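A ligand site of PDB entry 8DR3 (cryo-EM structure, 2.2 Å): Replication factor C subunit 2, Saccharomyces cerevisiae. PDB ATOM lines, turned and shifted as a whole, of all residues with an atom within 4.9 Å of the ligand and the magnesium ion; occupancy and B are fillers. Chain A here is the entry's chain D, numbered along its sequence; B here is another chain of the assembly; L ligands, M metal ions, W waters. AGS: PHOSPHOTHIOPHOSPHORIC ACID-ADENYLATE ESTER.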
ATOM      1  N   TRP A  27      -8.909  10.254 -33.598  1.00  0.00           N
ATOM      2  CA  TRP A  27      -9.366   9.011 -34.207  1.00  0.00           C
ATOM      3  C   TRP A  27      -9.379   7.855 -33.212  1.00  0.00           C
ATOM      4  O   TRP A  27     -10.246   6.976 -33.305  1.00  0.00           O
ATOM      5  CB  TRP A  27      -8.472   8.660 -35.408  1.00  0.00           C
ATOM      6  CG  TRP A  27      -8.674   9.565 -36.589  1.00  0.00           C
ATOM      7  CD1 TRP A  27      -9.380  10.738 -36.610  1.00  0.00           C
ATOM      8  CD2 TRP A  27      -8.164   9.368 -37.912  1.00  0.00           C
ATOM      9  NE1 TRP A  27      -9.341  11.277 -37.872  1.00  0.00           N
ATOM     10  CE2 TRP A  27      -8.598  10.465 -38.693  1.00  0.00           C
ATOM     11  CE3 TRP A  27      -7.388   8.381 -38.521  1.00  0.00           C
ATOM     12  CZ2 TRP A  27      -8.280  10.592 -40.037  1.00  0.00           C
ATOM     13  CZ3 TRP A  27      -7.072   8.509 -39.855  1.00  0.00           C
ATOM     14  CH2 TRP A  27      -7.521   9.609 -40.609  1.00  0.00           C
ATOM     15  N   VAL A  28      -8.447   7.835 -32.262  1.00  0.00           N
ATOM     16  CA  VAL A  28      -8.423   6.741 -31.280  1.00  0.00           C
ATOM     17  C   VAL A  28      -9.712   6.737 -30.475  1.00  0.00           C
ATOM     18  O   VAL A  28     -10.310   5.678 -30.246  1.00  0.00           O
ATOM     19  CB  VAL A  28      -7.180   6.860 -30.379  1.00  0.00           C
ATOM     20  CG1 VAL A  28      -5.916   6.618 -31.187  1.00  0.00           C
ATOM     21  CG2 VAL A  28      -7.129   8.207 -29.672  1.00  0.00           C
ATOM     22  N   GLU A  29     -10.161   7.905 -30.024  1.00  0.00           N
ATOM     23  CA  GLU A  29     -11.436   7.998 -29.319  1.00  0.00           C
ATOM     24  C   GLU A  29     -12.616   7.935 -30.269  1.00  0.00           C
ATOM     25  O   GLU A  29     -13.667   7.368 -29.922  1.00  0.00           O
ATOM     26  CB  GLU A  29     -11.498   9.282 -28.492  1.00  0.00           C
ATOM     27  CG  GLU A  29     -10.362   9.431 -27.491  1.00  0.00           C
ATOM     28  CD  GLU A  29     -10.419   8.400 -26.383  1.00  0.00           C
ATOM     29  OE1 GLU A  29     -11.364   7.573 -26.370  1.00  0.00           O
ATOM     30  OE2 GLU A  29      -9.518   8.396 -25.512  1.00  0.00           O
ATOM     31  N   TYR A  31     -13.007   6.220 -33.047  1.00  0.00           N
ATOM     32  CA  TYR A  31     -13.262   4.865 -33.520  1.00  0.00           C
ATOM     33  C   TYR A  31     -13.147   3.826 -32.418  1.00  0.00           C
ATOM     34  O   TYR A  31     -12.875   2.656 -32.701  1.00  0.00           O
ATOM     35  CB  TYR A  31     -12.304   4.541 -34.668  1.00  0.00           C
ATOM     36  CG  TYR A  31     -12.656   5.240 -35.960  1.00  0.00           C
ATOM     37  CD1 TYR A  31     -13.674   4.750 -36.772  1.00  0.00           C
ATOM     38  CD2 TYR A  31     -12.000   6.395 -36.352  1.00  0.00           C
ATOM     39  CE1 TYR A  31     -14.016   5.395 -37.950  1.00  0.00           C
ATOM     40  CE2 TYR A  31     -12.323   7.033 -37.526  1.00  0.00           C
ATOM     41  CZ  TYR A  31     -13.337   6.530 -38.326  1.00  0.00           C
ATOM     42  OH  TYR A  31     -13.671   7.172 -39.492  1.00  0.00           O
ATOM     43  N   ARG A  32     -13.362   4.222 -31.168  1.00  0.00           N
ATOM     44  CA  ARG A  32     -13.394   3.237 -30.096  1.00  0.00           C
ATOM     45  C   ARG A  32     -14.564   2.283 -30.323  1.00  0.00           C
ATOM     46  O   ARG A  32     -15.658   2.725 -30.696  1.00  0.00           O
ATOM     47  CB  ARG A  32     -13.546   3.932 -28.732  1.00  0.00           C
ATOM     48  CG  ARG A  32     -13.666   2.971 -27.557  1.00  0.00           C
ATOM     49  CD  ARG A  32     -13.779   3.719 -26.236  1.00  0.00           C
ATOM     50  NE  ARG A  32     -12.615   4.544 -25.948  1.00  0.00           N
ATOM     51  CZ  ARG A  32     -11.494   4.092 -25.406  1.00  0.00           C
ATOM     52  NH1 ARG A  32     -11.330   2.823 -25.089  1.00  0.00           N
ATOM     53  NH2 ARG A  32     -10.502   4.949 -25.175  1.00  0.00           N
ATOM     54  N   PRO A  33     -14.379   0.972 -30.124  1.00  0.00           N
ATOM     55  CA  PRO A  33     -15.487   0.039 -30.348  1.00  0.00           C
ATOM     56  C   PRO A  33     -16.689   0.393 -29.487  1.00  0.00           C
ATOM     57  O   PRO A  33     -16.559   0.768 -28.318  1.00  0.00           O
ATOM     58  CB  PRO A  33     -14.894  -1.322 -29.961  1.00  0.00           C
ATOM     59  CG  PRO A  33     -13.428  -1.156 -29.985  1.00  0.00           C
ATOM     60  CD  PRO A  33     -13.126   0.283 -29.747  1.00  0.00           C
ATOM     61  N   GLU A  38     -17.183  -5.167 -32.528  1.00  0.00           N
ATOM     62  CA  GLU A  38     -16.182  -4.279 -33.112  1.00  0.00           C
ATOM     63  C   GLU A  38     -14.782  -4.522 -32.554  1.00  0.00           C
ATOM     64  O   GLU A  38     -13.839  -3.858 -32.995  1.00  0.00           O
ATOM     65  CB  GLU A  38     -16.575  -2.818 -32.886  1.00  0.00           C
ATOM     66  CG  GLU A  38     -17.761  -2.356 -33.717  1.00  0.00           C
ATOM     67  CD  GLU A  38     -17.957  -0.855 -33.685  1.00  0.00           C
ATOM     68  OE1 GLU A  38     -18.086  -0.300 -32.572  1.00  0.00           O
ATOM     69  OE2 GLU A  38     -17.969  -0.227 -34.754  1.00  0.00           O
ATOM     70  N   VAL A  39     -14.623  -5.448 -31.617  1.00  0.00           N
ATOM     71  CA  VAL A  39     -13.299  -5.819 -31.125  1.00  0.00           C
ATOM     72  C   VAL A  39     -12.643  -6.724 -32.158  1.00  0.00           C
ATOM     73  O   VAL A  39     -13.244  -7.705 -32.603  1.00  0.00           O
ATOM     74  CB  VAL A  39     -13.399  -6.492 -29.753  1.00  0.00           C
ATOM     75  CG1 VAL A  39     -12.015  -6.773 -29.187  1.00  0.00           C
ATOM     76  CG2 VAL A  39     -14.210  -5.634 -28.792  1.00  0.00           C
ATOM     77  N   THR A  40     -11.402  -6.415 -32.514  1.00  0.00           N
ATOM     78  CA  THR A  40     -10.814  -6.964 -33.737  1.00  0.00           C
ATOM     79  C   THR A  40     -10.313  -8.395 -33.553  1.00  0.00           C
ATOM     80  O   THR A  40     -10.837  -9.327 -34.177  1.00  0.00           O
ATOM     81  CB  THR A  40      -9.670  -6.070 -34.220  1.00  0.00           C
ATOM     82  OG1 THR A  40     -10.128  -4.713 -34.323  1.00  0.00           O
ATOM     83  CG2 THR A  40      -9.166  -6.539 -35.573  1.00  0.00           C
ATOM     84  N   ALA A  41      -9.317  -8.591 -32.691  1.00  0.00           N
ATOM     85  CA  ALA A  41      -8.557  -9.848 -32.658  1.00  0.00           C
ATOM     86  C   ALA A  41      -8.443 -10.377 -31.232  1.00  0.00           C
ATOM     87  O   ALA A  41      -7.376 -10.793 -30.783  1.00  0.00           O
ATOM     88  CB  ALA A  41      -7.174  -9.646 -33.261  1.00  0.00           C
ATOM     89  N   GLN A  42      -9.558 -10.373 -30.514  1.00  0.00           N
ATOM     90  CA  GLN A  42      -9.633 -10.926 -29.158  1.00  0.00           C
ATOM     91  C   GLN A  42     -10.803 -11.902 -29.058  1.00  0.00           C
ATOM     92  O   GLN A  42     -11.530 -11.926 -28.065  1.00  0.00           O
ATOM     93  CB  GLN A  42      -9.757  -9.815 -28.128  1.00  0.00           C
ATOM     94  CG  GLN A  42      -8.786  -8.657 -28.311  1.00  0.00           C
ATOM     95  CD  GLN A  42      -7.334  -9.047 -28.048  1.00  0.00           C
ATOM     96  OE1 GLN A  42      -7.027 -10.221 -27.834  1.00  0.00           O
ATOM     97  NE2 GLN A  42      -6.449  -8.062 -28.064  1.00  0.00           N
ATOM     98  N   GLY A  65      -2.990  -7.428 -20.332  1.00  0.00           N
ATOM     99  CA  GLY A  65      -2.324  -7.353 -21.614  1.00  0.00           C
ATOM    100  C   GLY A  65      -1.548  -6.071 -21.838  1.00  0.00           C
ATOM    101  O   GLY A  65      -1.616  -5.123 -21.051  1.00  0.00           O
ATOM    102  N   PRO A  66      -0.810  -6.023 -22.941  1.00  0.00           N
ATOM    103  CA  PRO A  66       0.036  -4.856 -23.232  1.00  0.00           C
ATOM    104  C   PRO A  66      -0.794  -3.655 -23.647  1.00  0.00           C
ATOM    105  O   PRO A  66      -2.007  -3.786 -23.888  1.00  0.00           O
ATOM    106  CB  PRO A  66       0.936  -5.340 -24.380  1.00  0.00           C
ATOM    107  CG  PRO A  66       0.156  -6.424 -25.036  1.00  0.00           C
ATOM    108  CD  PRO A  66      -0.675  -7.074 -23.969  1.00  0.00           C
ATOM    109  N   PRO A  67      -0.185  -2.483 -23.731  1.00  0.00           N
ATOM    110  CA  PRO A  67      -0.963  -1.257 -23.992  1.00  0.00           C
ATOM    111  C   PRO A  67      -1.710  -1.299 -25.312  1.00  0.00           C
ATOM    112  O   PRO A  67      -1.236  -1.877 -26.303  1.00  0.00           O
ATOM    113  CB  PRO A  67       0.106  -0.146 -23.991  1.00  0.00           C
ATOM    114  CG  PRO A  67       1.288  -0.725 -23.293  1.00  0.00           C
ATOM    115  CD  PRO A  67       1.250  -2.192 -23.547  1.00  0.00           C
ATOM    116  N   GLY A  68      -2.883  -0.684 -25.324  1.00  0.00           N
ATOM    117  CA  GLY A  68      -3.653  -0.491 -26.537  1.00  0.00           C
ATOM    118  C   GLY A  68      -4.082  -1.782 -27.211  1.00  0.00           C
ATOM    119  O   GLY A  68      -3.946  -1.907 -28.438  1.00  0.00           O
ATOM    120  N   THR A  69      -4.592  -2.737 -26.443  1.00  0.00           N
ATOM    121  CA  THR A  69      -5.061  -4.002 -26.983  1.00  0.00           C
ATOM    122  C   THR A  69      -6.577  -4.151 -26.949  1.00  0.00           C
ATOM    123  O   THR A  69      -7.103  -5.070 -27.595  1.00  0.00           O
ATOM    124  CB  THR A  69      -4.435  -5.176 -26.222  1.00  0.00           C
ATOM    125  OG1 THR A  69      -4.313  -4.845 -24.830  1.00  0.00           O
ATOM    126  CG2 THR A  69      -3.056  -5.496 -26.782  1.00  0.00           C
ATOM    127  N   GLY A  70      -7.293  -3.289 -26.225  1.00  0.00           N
ATOM    128  CA  GLY A  70      -8.747  -3.297 -26.241  1.00  0.00           C
ATOM    129  C   GLY A  70      -9.395  -3.844 -24.984  1.00  0.00           C
ATOM    130  O   GLY A  70     -10.460  -4.453 -25.058  1.00  0.00           O
ATOM    131  N   LYS A  71      -8.764  -3.623 -23.832  1.00  0.00           N
ATOM    132  CA  LYS A  71      -9.308  -4.121 -22.574  1.00  0.00           C
ATOM    133  C   LYS A  71     -10.413  -3.216 -22.043  1.00  0.00           C
ATOM    134  O   LYS A  71     -11.539  -3.655 -21.784  1.00  0.00           O
ATOM    135  CB  LYS A  71      -8.179  -4.269 -21.541  1.00  0.00           C
ATOM    136  CG  LYS A  71      -6.999  -5.097 -22.037  1.00  0.00           C
ATOM    137  CD  LYS A  71      -6.013  -5.402 -20.911  1.00  0.00           C
ATOM    138  CE  LYS A  71      -5.078  -4.231 -20.632  1.00  0.00           C
ATOM    139  NZ  LYS A  71      -4.356  -3.746 -21.833  1.00  0.00           N
ATOM    140  N   THR A  72     -10.103  -1.923 -21.884  1.00  0.00           N
ATOM    141  CA  THR A  72     -11.099  -0.967 -21.423  1.00  0.00           C
ATOM    142  C   THR A  72     -12.270  -0.903 -22.402  1.00  0.00           C
ATOM    143  O   THR A  72     -13.440  -0.870 -21.991  1.00  0.00           O
ATOM    144  CB  THR A  72     -10.458   0.411 -21.247  1.00  0.00           C
ATOM    145  OG1 THR A  72      -9.648   0.419 -20.077  1.00  0.00           O
ATOM    146  CG2 THR A  72     -11.531   1.492 -21.129  1.00  0.00           C
ATOM    147  N   SER A  73     -11.977  -0.877 -23.699  1.00  0.00           N
ATOM    148  CA  SER A  73     -13.039  -0.882 -24.696  1.00  0.00           C
ATOM    149  C   SER A  73     -13.903  -2.128 -24.562  1.00  0.00           C
ATOM    150  O   SER A  73     -15.126  -2.053 -24.653  1.00  0.00           O
ATOM    151  CB  SER A  73     -12.435  -0.809 -26.103  1.00  0.00           C
ATOM    152  OG  SER A  73     -11.633   0.343 -26.260  1.00  0.00           O
ATOM    153  N   ASP A 140     -10.031  -0.487 -13.114  1.00  0.00           N
ATOM    154  CA  ASP A 140      -9.056  -0.301 -14.179  1.00  0.00           C
ATOM    155  C   ASP A 140      -7.702   0.086 -13.594  1.00  0.00           C
ATOM    156  O   ASP A 140      -7.616   0.762 -12.569  1.00  0.00           O
ATOM    157  CB  ASP A 140      -9.530   0.780 -15.152  1.00  0.00           C
ATOM    158  CG  ASP A 140      -9.100   0.513 -16.583  1.00  0.00           C
ATOM    159  OD1 ASP A 140      -8.210  -0.349 -16.791  1.00  0.00           O
ATOM    160  OD2 ASP A 140      -9.649   1.150 -17.508  1.00  0.00           O
ATOM    161  N   GLU A 141      -6.640  -0.359 -14.259  1.00  0.00           N
ATOM    162  CA  GLU A 141      -5.281  -0.159 -13.763  1.00  0.00           C
ATOM    163  C   GLU A 141      -5.132  -0.720 -12.350  1.00  0.00           C
ATOM    164  O   GLU A 141      -4.535  -0.097 -11.474  1.00  0.00           O
ATOM    165  CB  GLU A 141      -4.892   1.322 -13.814  1.00  0.00           C
ATOM    166  CG  GLU A 141      -4.680   1.863 -15.223  1.00  0.00           C
ATOM    167  CD  GLU A 141      -5.595   3.025 -15.564  1.00  0.00           C
ATOM    168  OE1 GLU A 141      -5.990   3.782 -14.639  1.00  0.00           O
ATOM    169  OE2 GLU A 141      -5.925   3.189 -16.757  1.00  0.00           O
ATOM    170  N   ASN A 171      -1.843  -4.217 -17.049  1.00  0.00           N
ATOM    171  CA  ASN A 171      -0.776  -4.486 -18.000  1.00  0.00           C
ATOM    172  C   ASN A 171       0.251  -5.477 -17.484  1.00  0.00           C
ATOM    173  O   ASN A 171       0.851  -6.197 -18.285  1.00  0.00           O
ATOM    174  CB  ASN A 171      -0.059  -3.184 -18.369  1.00  0.00           C
ATOM    175  CG  ASN A 171      -0.955  -2.222 -19.144  1.00  0.00           C
ATOM    176  OD1 ASN A 171      -1.145  -1.078 -18.730  1.00  0.00           O
ATOM    177  ND2 ASN A 171      -1.495  -2.679 -20.264  1.00  0.00           N
ATOM    178  N   LEU A 192      -1.604  -6.730 -31.038  1.00  0.00           N
ATOM    179  CA  LEU A 192      -2.253  -6.480 -32.318  1.00  0.00           C
ATOM    180  C   LEU A 192      -1.180  -6.129 -33.354  1.00  0.00           C
ATOM    181  O   LEU A 192      -0.543  -5.074 -33.258  1.00  0.00           O
ATOM    182  CB  LEU A 192      -3.278  -5.352 -32.191  1.00  0.00           C
ATOM    183  CG  LEU A 192      -4.389  -5.604 -31.164  1.00  0.00           C
ATOM    184  CD1 LEU A 192      -5.251  -4.367 -31.003  1.00  0.00           C
ATOM    185  CD2 LEU A 192      -5.225  -6.804 -31.545  1.00  0.00           C
ATOM    186  N   ARG A 200      -9.145  -3.792 -39.262  1.00  0.00           N
ATOM    187  CA  ARG A 200      -9.674  -2.622 -38.582  1.00  0.00           C
ATOM    188  C   ARG A 200      -9.003  -1.338 -39.074  1.00  0.00           C
ATOM    189  O   ARG A 200      -9.672  -0.323 -39.290  1.00  0.00           O
ATOM    190  CB  ARG A 200      -9.505  -2.772 -37.065  1.00  0.00           C
ATOM    191  CG  ARG A 200     -10.078  -1.616 -36.251  1.00  0.00           C
ATOM    192  CD  ARG A 200     -11.579  -1.503 -36.401  1.00  0.00           C
ATOM    193  NE  ARG A 200     -12.149  -0.524 -35.494  1.00  0.00           N
ATOM    194  CZ  ARG A 200     -13.425  -0.151 -35.485  1.00  0.00           C
ATOM    195  NH1 ARG A 200     -14.305  -0.666 -36.329  1.00  0.00           N
ATOM    196  NH2 ARG A 200     -13.827   0.771 -34.604  1.00  0.00           N
ATOM    197  N   LEU A 228      -2.415  -0.923 -31.170  1.00  0.00           N
ATOM    198  CA  LEU A 228      -3.283  -0.399 -32.222  1.00  0.00           C
ATOM    199  C   LEU A 228      -3.586   1.085 -32.018  1.00  0.00           C
ATOM    200  O   LEU A 228      -3.811   1.814 -32.988  1.00  0.00           O
ATOM    201  CB  LEU A 228      -4.592  -1.189 -32.274  1.00  0.00           C
ATOM    202  CG  LEU A 228      -5.607  -0.781 -33.346  1.00  0.00           C
ATOM    203  CD1 LEU A 228      -4.941  -0.668 -34.720  1.00  0.00           C
ATOM    204  CD2 LEU A 228      -6.759  -1.764 -33.396  1.00  0.00           C
ATOM    205  N   ARG A 229      -3.576   1.561 -30.773  1.00  0.00           N
ATOM    206  CA  ARG A 229      -3.772   2.983 -30.515  1.00  0.00           C
ATOM    207  C   ARG A 229      -2.671   3.808 -31.170  1.00  0.00           C
ATOM    208  O   ARG A 229      -2.932   4.825 -31.823  1.00  0.00           O
ATOM    209  CB  ARG A 229      -3.813   3.236 -29.004  1.00  0.00           C
ATOM    210  CG  ARG A 229      -4.402   4.585 -28.603  1.00  0.00           C
ATOM    211  CD  ARG A 229      -3.966   5.007 -27.207  1.00  0.00           C
ATOM    212  NE  ARG A 229      -4.836   4.468 -26.170  1.00  0.00           N
ATOM    213  CZ  ARG A 229      -4.494   3.544 -25.276  1.00  0.00           C
ATOM    214  NH1 ARG A 229      -3.284   3.001 -25.266  1.00  0.00           N
ATOM    215  NH2 ARG A 229      -5.380   3.157 -24.365  1.00  0.00           N
ATOM    216  N   ILE A 232      -3.217   3.841 -34.971  1.00  0.00           N
ATOM    217  CA  ILE A 232      -4.281   4.763 -35.381  1.00  0.00           C
ATOM    218  C   ILE A 232      -3.791   6.210 -35.298  1.00  0.00           C
ATOM    219  O   ILE A 232      -4.077   7.028 -36.180  1.00  0.00           O
ATOM    220  CB  ILE A 232      -5.540   4.533 -34.539  1.00  0.00           C
ATOM    221  CG1 ILE A 232      -6.176   3.187 -34.887  1.00  0.00           C
ATOM    222  CG2 ILE A 232      -6.537   5.663 -34.752  1.00  0.00           C
ATOM    223  CD1 ILE A 232      -7.108   2.646 -33.821  1.00  0.00           C
ATOM    224  N   ARG B 155      -3.385   8.543 -17.098  1.00  0.00           N
ATOM    225  CA  ARG B 155      -3.781   7.583 -18.125  1.00  0.00           C
ATOM    226  C   ARG B 155      -5.251   7.755 -18.523  1.00  0.00           C
ATOM    227  O   ARG B 155      -5.560   8.089 -19.672  1.00  0.00           O
ATOM    228  CB  ARG B 155      -3.538   6.158 -17.627  1.00  0.00           C
ATOM    229  CG  ARG B 155      -2.089   5.717 -17.701  1.00  0.00           C
ATOM    230  CD  ARG B 155      -1.884   4.349 -17.078  1.00  0.00           C
ATOM    231  NE  ARG B 155      -2.702   3.320 -17.712  1.00  0.00           N
ATOM    232  CZ  ARG B 155      -2.403   2.026 -17.723  1.00  0.00           C
ATOM    233  NH1 ARG B 155      -1.298   1.568 -17.164  1.00  0.00           N
ATOM    234  NH2 ARG B 155      -3.226   1.177 -18.329  1.00  0.00           N
ATOM    235  N   GLU B 159      -8.086  10.083 -21.588  1.00  0.00           N
ATOM    236  CA  GLU B 159      -9.051   9.408 -22.459  1.00  0.00           C
ATOM    237  C   GLU B 159     -10.479   9.861 -22.207  1.00  0.00           C
ATOM    238  O   GLU B 159     -11.212  10.162 -23.157  1.00  0.00           O
ATOM    239  CB  GLU B 159      -8.937   7.891 -22.283  1.00  0.00           C
ATOM    240  CG  GLU B 159      -7.646   7.291 -22.808  1.00  0.00           C
ATOM    241  CD  GLU B 159      -7.661   5.776 -22.792  1.00  0.00           C
ATOM    242  OE1 GLU B 159      -7.863   5.200 -21.696  1.00  0.00           O
ATOM    243  OE2 GLU B 159      -7.466   5.163 -23.860  1.00  0.00           O
ATOM    244  N   PRO B 180       2.116   3.285 -21.388  1.00  0.00           N
ATOM    245  CA  PRO B 180       0.746   3.724 -21.696  1.00  0.00           C
ATOM    246  C   PRO B 180       0.646   5.187 -22.083  1.00  0.00           C
ATOM    247  O   PRO B 180      -0.107   5.535 -23.008  1.00  0.00           O
ATOM    248  CB  PRO B 180      -0.020   3.417 -20.393  1.00  0.00           C
ATOM    249  CG  PRO B 180       0.790   2.375 -19.707  1.00  0.00           C
ATOM    250  CD  PRO B 180       2.215   2.652 -20.067  1.00  0.00           C
ATOM    251  N   ARG B 184      -0.619   6.907 -25.573  1.00  0.00           N
ATOM    252  CA  ARG B 184      -1.724   7.849 -25.594  1.00  0.00           C
ATOM    253  C   ARG B 184      -1.382   9.175 -26.256  1.00  0.00           C
ATOM    254  O   ARG B 184      -2.258  10.043 -26.362  1.00  0.00           O
ATOM    255  CB  ARG B 184      -2.219   8.109 -24.177  1.00  0.00           C
ATOM    256  CG  ARG B 184      -3.205   7.082 -23.650  1.00  0.00           C
ATOM    257  CD  ARG B 184      -3.401   7.230 -22.150  1.00  0.00           C
ATOM    258  NE  ARG B 184      -4.463   6.369 -21.640  1.00  0.00           N
ATOM    259  CZ  ARG B 184      -4.342   5.061 -21.444  1.00  0.00           C
ATOM    260  NH1 ARG B 184      -3.216   4.427 -21.706  1.00  0.00           N
ATOM    261  NH2 ARG B 184      -5.384   4.376 -20.982  1.00  0.00           N
HETATM  262  PG  AGS L   1      -4.196   0.429 -21.733  1.00  0.00           P
HETATM  263  S1G AGS L   1      -2.505   1.279 -22.050  1.00  0.00           S
HETATM  264  O2G AGS L   1      -5.067   1.343 -20.643  1.00  0.00           O
HETATM  265  O3G AGS L   1      -3.966  -1.116 -21.124  1.00  0.00           O
HETATM  266  PB  AGS L   1      -6.213  -0.739 -23.514  1.00  0.00           P
HETATM  267  O1B AGS L   1      -5.649  -2.149 -23.490  1.00  0.00           O
HETATM  268  O2B AGS L   1      -7.338  -0.623 -22.502  1.00  0.00           O
HETATM  269  O3B AGS L   1      -5.030   0.361 -23.152  1.00  0.00           O
HETATM  270  PA  AGS L   1      -8.073   0.481 -25.297  1.00  0.00           P
HETATM  271  O1A AGS L   1      -9.290  -0.351 -25.034  1.00  0.00           O
HETATM  272  O2A AGS L   1      -8.093   1.704 -24.419  1.00  0.00           O
HETATM  273  O3A AGS L   1      -6.751  -0.396 -25.006  1.00  0.00           O
HETATM  274  O5' AGS L   1      -8.047   0.962 -26.908  1.00  0.00           O
HETATM  275  C5' AGS L   1      -7.603   2.239 -27.211  1.00  0.00           C
HETATM  276  C4' AGS L   1      -7.949   2.562 -28.623  1.00  0.00           C
HETATM  277  O4' AGS L   1      -7.187   1.882 -29.452  1.00  0.00           O
HETATM  278  C3' AGS L   1      -9.528   2.138 -28.918  1.00  0.00           C
HETATM  279  O3' AGS L   1     -10.403   3.329 -28.780  1.00  0.00           O
HETATM  280  C2' AGS L   1      -9.562   1.708 -30.077  1.00  0.00           C
HETATM  281  O2' AGS L   1      -9.779   2.825 -31.027  1.00  0.00           O
HETATM  282  C1' AGS L   1      -8.107   1.064 -30.322  1.00  0.00           C
HETATM  283  N9  AGS L   1      -8.024  -0.222 -29.960  1.00  0.00           N
HETATM  284  C8  AGS L   1      -7.258  -0.858 -29.082  1.00  0.00           C
HETATM  285  N7  AGS L   1      -7.573  -2.157 -29.119  1.00  0.00           N
HETATM  286  C5  AGS L   1      -8.528  -2.324 -30.032  1.00  0.00           C
HETATM  287  C6  AGS L   1      -9.210  -3.435 -30.473  1.00  0.00           C
HETATM  288  N6  AGS L   1      -9.013  -4.821 -30.005  1.00  0.00           N
HETATM  289  N1  AGS L   1     -10.125  -3.327 -31.410  1.00  0.00           N
HETATM  290  C2  AGS L   1     -10.408  -2.119 -31.935  1.00  0.00           C
HETATM  291  N3  AGS L   1      -9.743  -1.033 -31.507  1.00  0.00           N
HETATM  292  C4  AGS L   1      -8.805  -1.129 -30.556  1.00  0.00           C
HETATM  293 MG    MG M   1      -7.230   0.885 -20.854  1.00  0.00          MG
HETATM  294  O   HOH W   1      -7.136   2.312 -18.872  1.00  0.00           O
HETATM  295  O   HOH W   2      -6.659  -0.600 -19.287  1.00  0.00           O
HETATM  296  O   HOH W   3      -7.752   2.325 -22.013  1.00  0.00           O
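The guanidinium group (NH1) of Arg 155 of chain B sits at hydrogen-bond distance from the side-chain amide oxygen (OD1) of Asn 171 (3.1 Å).
O of Gly 68 is in hydrogen-bond range of N of Leu 228, at 3.3 Å.
The backbone carbonyl oxygen (O) of Thr 69 is in hydrogen-bond range of the side-chain amide nitrogen (NE2) of Gln 42, 3.1 Å away.
The side-chain carboxylate (OE1) of Glu 159 of chain B lies within salt-bridge range of the guanidinium group (NH2) of Arg 184 of chain B.
ND2 of Asn 171 sits at hydrogen-bond distance from O of Gly 65 (2.6 Å).
NZ of Lys 71 lies close to ND2 of Asn 171 (3.4 Å).
The side-chain amino group of Lys 71 is in hydrogen-bond range of the backbone carbonyl oxygen of Gly 65 (3.2 Å).
OD2 of Asp 140 lies close to OG1 of Thr 72, at 2.7 Å.
The backbone carbonyl oxygen (O) of Val 28 lies within hydrogen-bond range of an oxygen (O3') of the ligand.
The side-chain hydroxyl (OG1) of Thr 69 is in hydrogen-bond range of an oxygen (O1B) of the ligand (3.3 Å).
O of Thr 69 lies within hydrogen-bond range of N6 of the ligand, at 3.1 Å.
The guanidinium group (NH1) of Arg 32 is in salt-bridge range of an oxygen (O2A) of the ligand, 3.5 Å away.
An oxygen (O1B) of the ligand lies within hydrogen-bond range of the backbone NH (N) of Lys 71.
The side-chain hydroxyl of Ser 73 sits at hydrogen-bond distance from an oxygen (O1A) of the ligand (2.7 Å).
The backbone NH of Ser 73 lies within hydrogen-bond range of an oxygen (O1A) of the ligand (3.0 Å).
N of Thr 69 is in hydrogen-bond range of O1B of the ligand (3.2 Å).
ND2 of Asn 171 sits at hydrogen-bond distance from O3G of the ligand (3.0 Å).
N of Thr 72 sits close to O2B of the ligand.
A sulfur (S1G) of the ligand sits close to the guanidinium group (NH2) of Arg 155 of chain B (3.8 Å).
The backbone NH (N) of Gly 70 sits at hydrogen-bond distance from a nitrogen (N7) of the ligand, 3.1 Å away.
O1B of the ligand is in salt-bridge range of NZ of Lys 71, 2.6 Å away.
N of Gly 68 lies within hydrogen-bond range of O3B of the ligand (3.2 Å).
NH2 of Arg 229 is in salt-bridge range of O2A of the ligand (3.1 Å).
OG1 of Thr 40 lies within hydrogen-bond range of N1 of the ligand, 3.2 Å away.
The guanidinium group of Arg 184 of chain B sits close to a sulfur (S1G) of the ligand (3.2 Å).
The magnesium ion is bound by water W3 (1.9 Å).
An oxygen (O2G) of the ligand is bound to the magnesium ion.
The magnesium ion is bound by water W2 (2.2 Å).
An oxygen (O2B) of the ligand is bound to the magnesium ion, at 2.2 Å.
Water W1 is bound to the magnesium ion (2.4 Å).
OG1 of Thr 72 is bound to the magnesium ion (2.6 Å).
The magnesium ion has six donor atoms within binding distance.
O of Tyr 31 touches O2' of the ligand (3.5 Å).
Pro 33 touches the ligand (CG to C2, 3.7 Å).
Glu 38 touches the ligand (O to C2, 3.99 Å).
Val 39 touches the ligand (CG1 to N6, 3.7 Å).
Pro 67 touches the ligand.
Leu 192 touches the ligand.
Leu 228 touches the ligand (CD2 to C4, 3.6 Å).
Ile 232 touches the ligand.
Glu 159 of chain B touches the ligand.
Pro 180 of chain B touches the ligand.
Hydrophobic or aromatic side chains within 4 Å of the ligand: Pro 33, Val 39, Pro 67, Leu 192, Leu 228, Ile 232 and Pro 180 of chain B.
Within 4 Å of the ligand: Val 28, Tyr 31, Arg 32, Pro 33, Glu 38, Val 39, Thr 40, Pro 67, Gly 68, Thr 69, Gly 70, Lys 71, Thr 72, Ser 73, Asn 171, Leu 192, Leu 228, Arg 229, Ile 232, Arg 155 of chain B, Glu 159 of chain B, Pro 180 of chain B and Arg 184 of chain B.
Arg 184 of chain B touches the magnesium ion (NH2 to MG, 3.95 Å).
Within 4 Å of the magnesium ion: Thr 72 and Arg 184 of chain B.
Water W3 lies within hydrogen-bond range of an oxygen (O2A) of the ligand, the side-chain carboxylate (OE1) of Glu 159 of chain B, the guanidinium group (NH2) of Arg 184 of chain B and the guanidinium group (NH2) of Arg 229.
Water W2 lies within hydrogen-bond range of the side-chain carboxylate of Asp 140 (2.9 Å) and an oxygen (O3G) of the ligand (3.3 Å).
Water W1 lies within hydrogen-bond range of the side-chain carboxylate of Glu 141 (2.6 Å), the side-chain carboxylate of Asp 140 (3.1 Å) and the guanidinium group of Arg 184 of chain B (3.4 Å).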
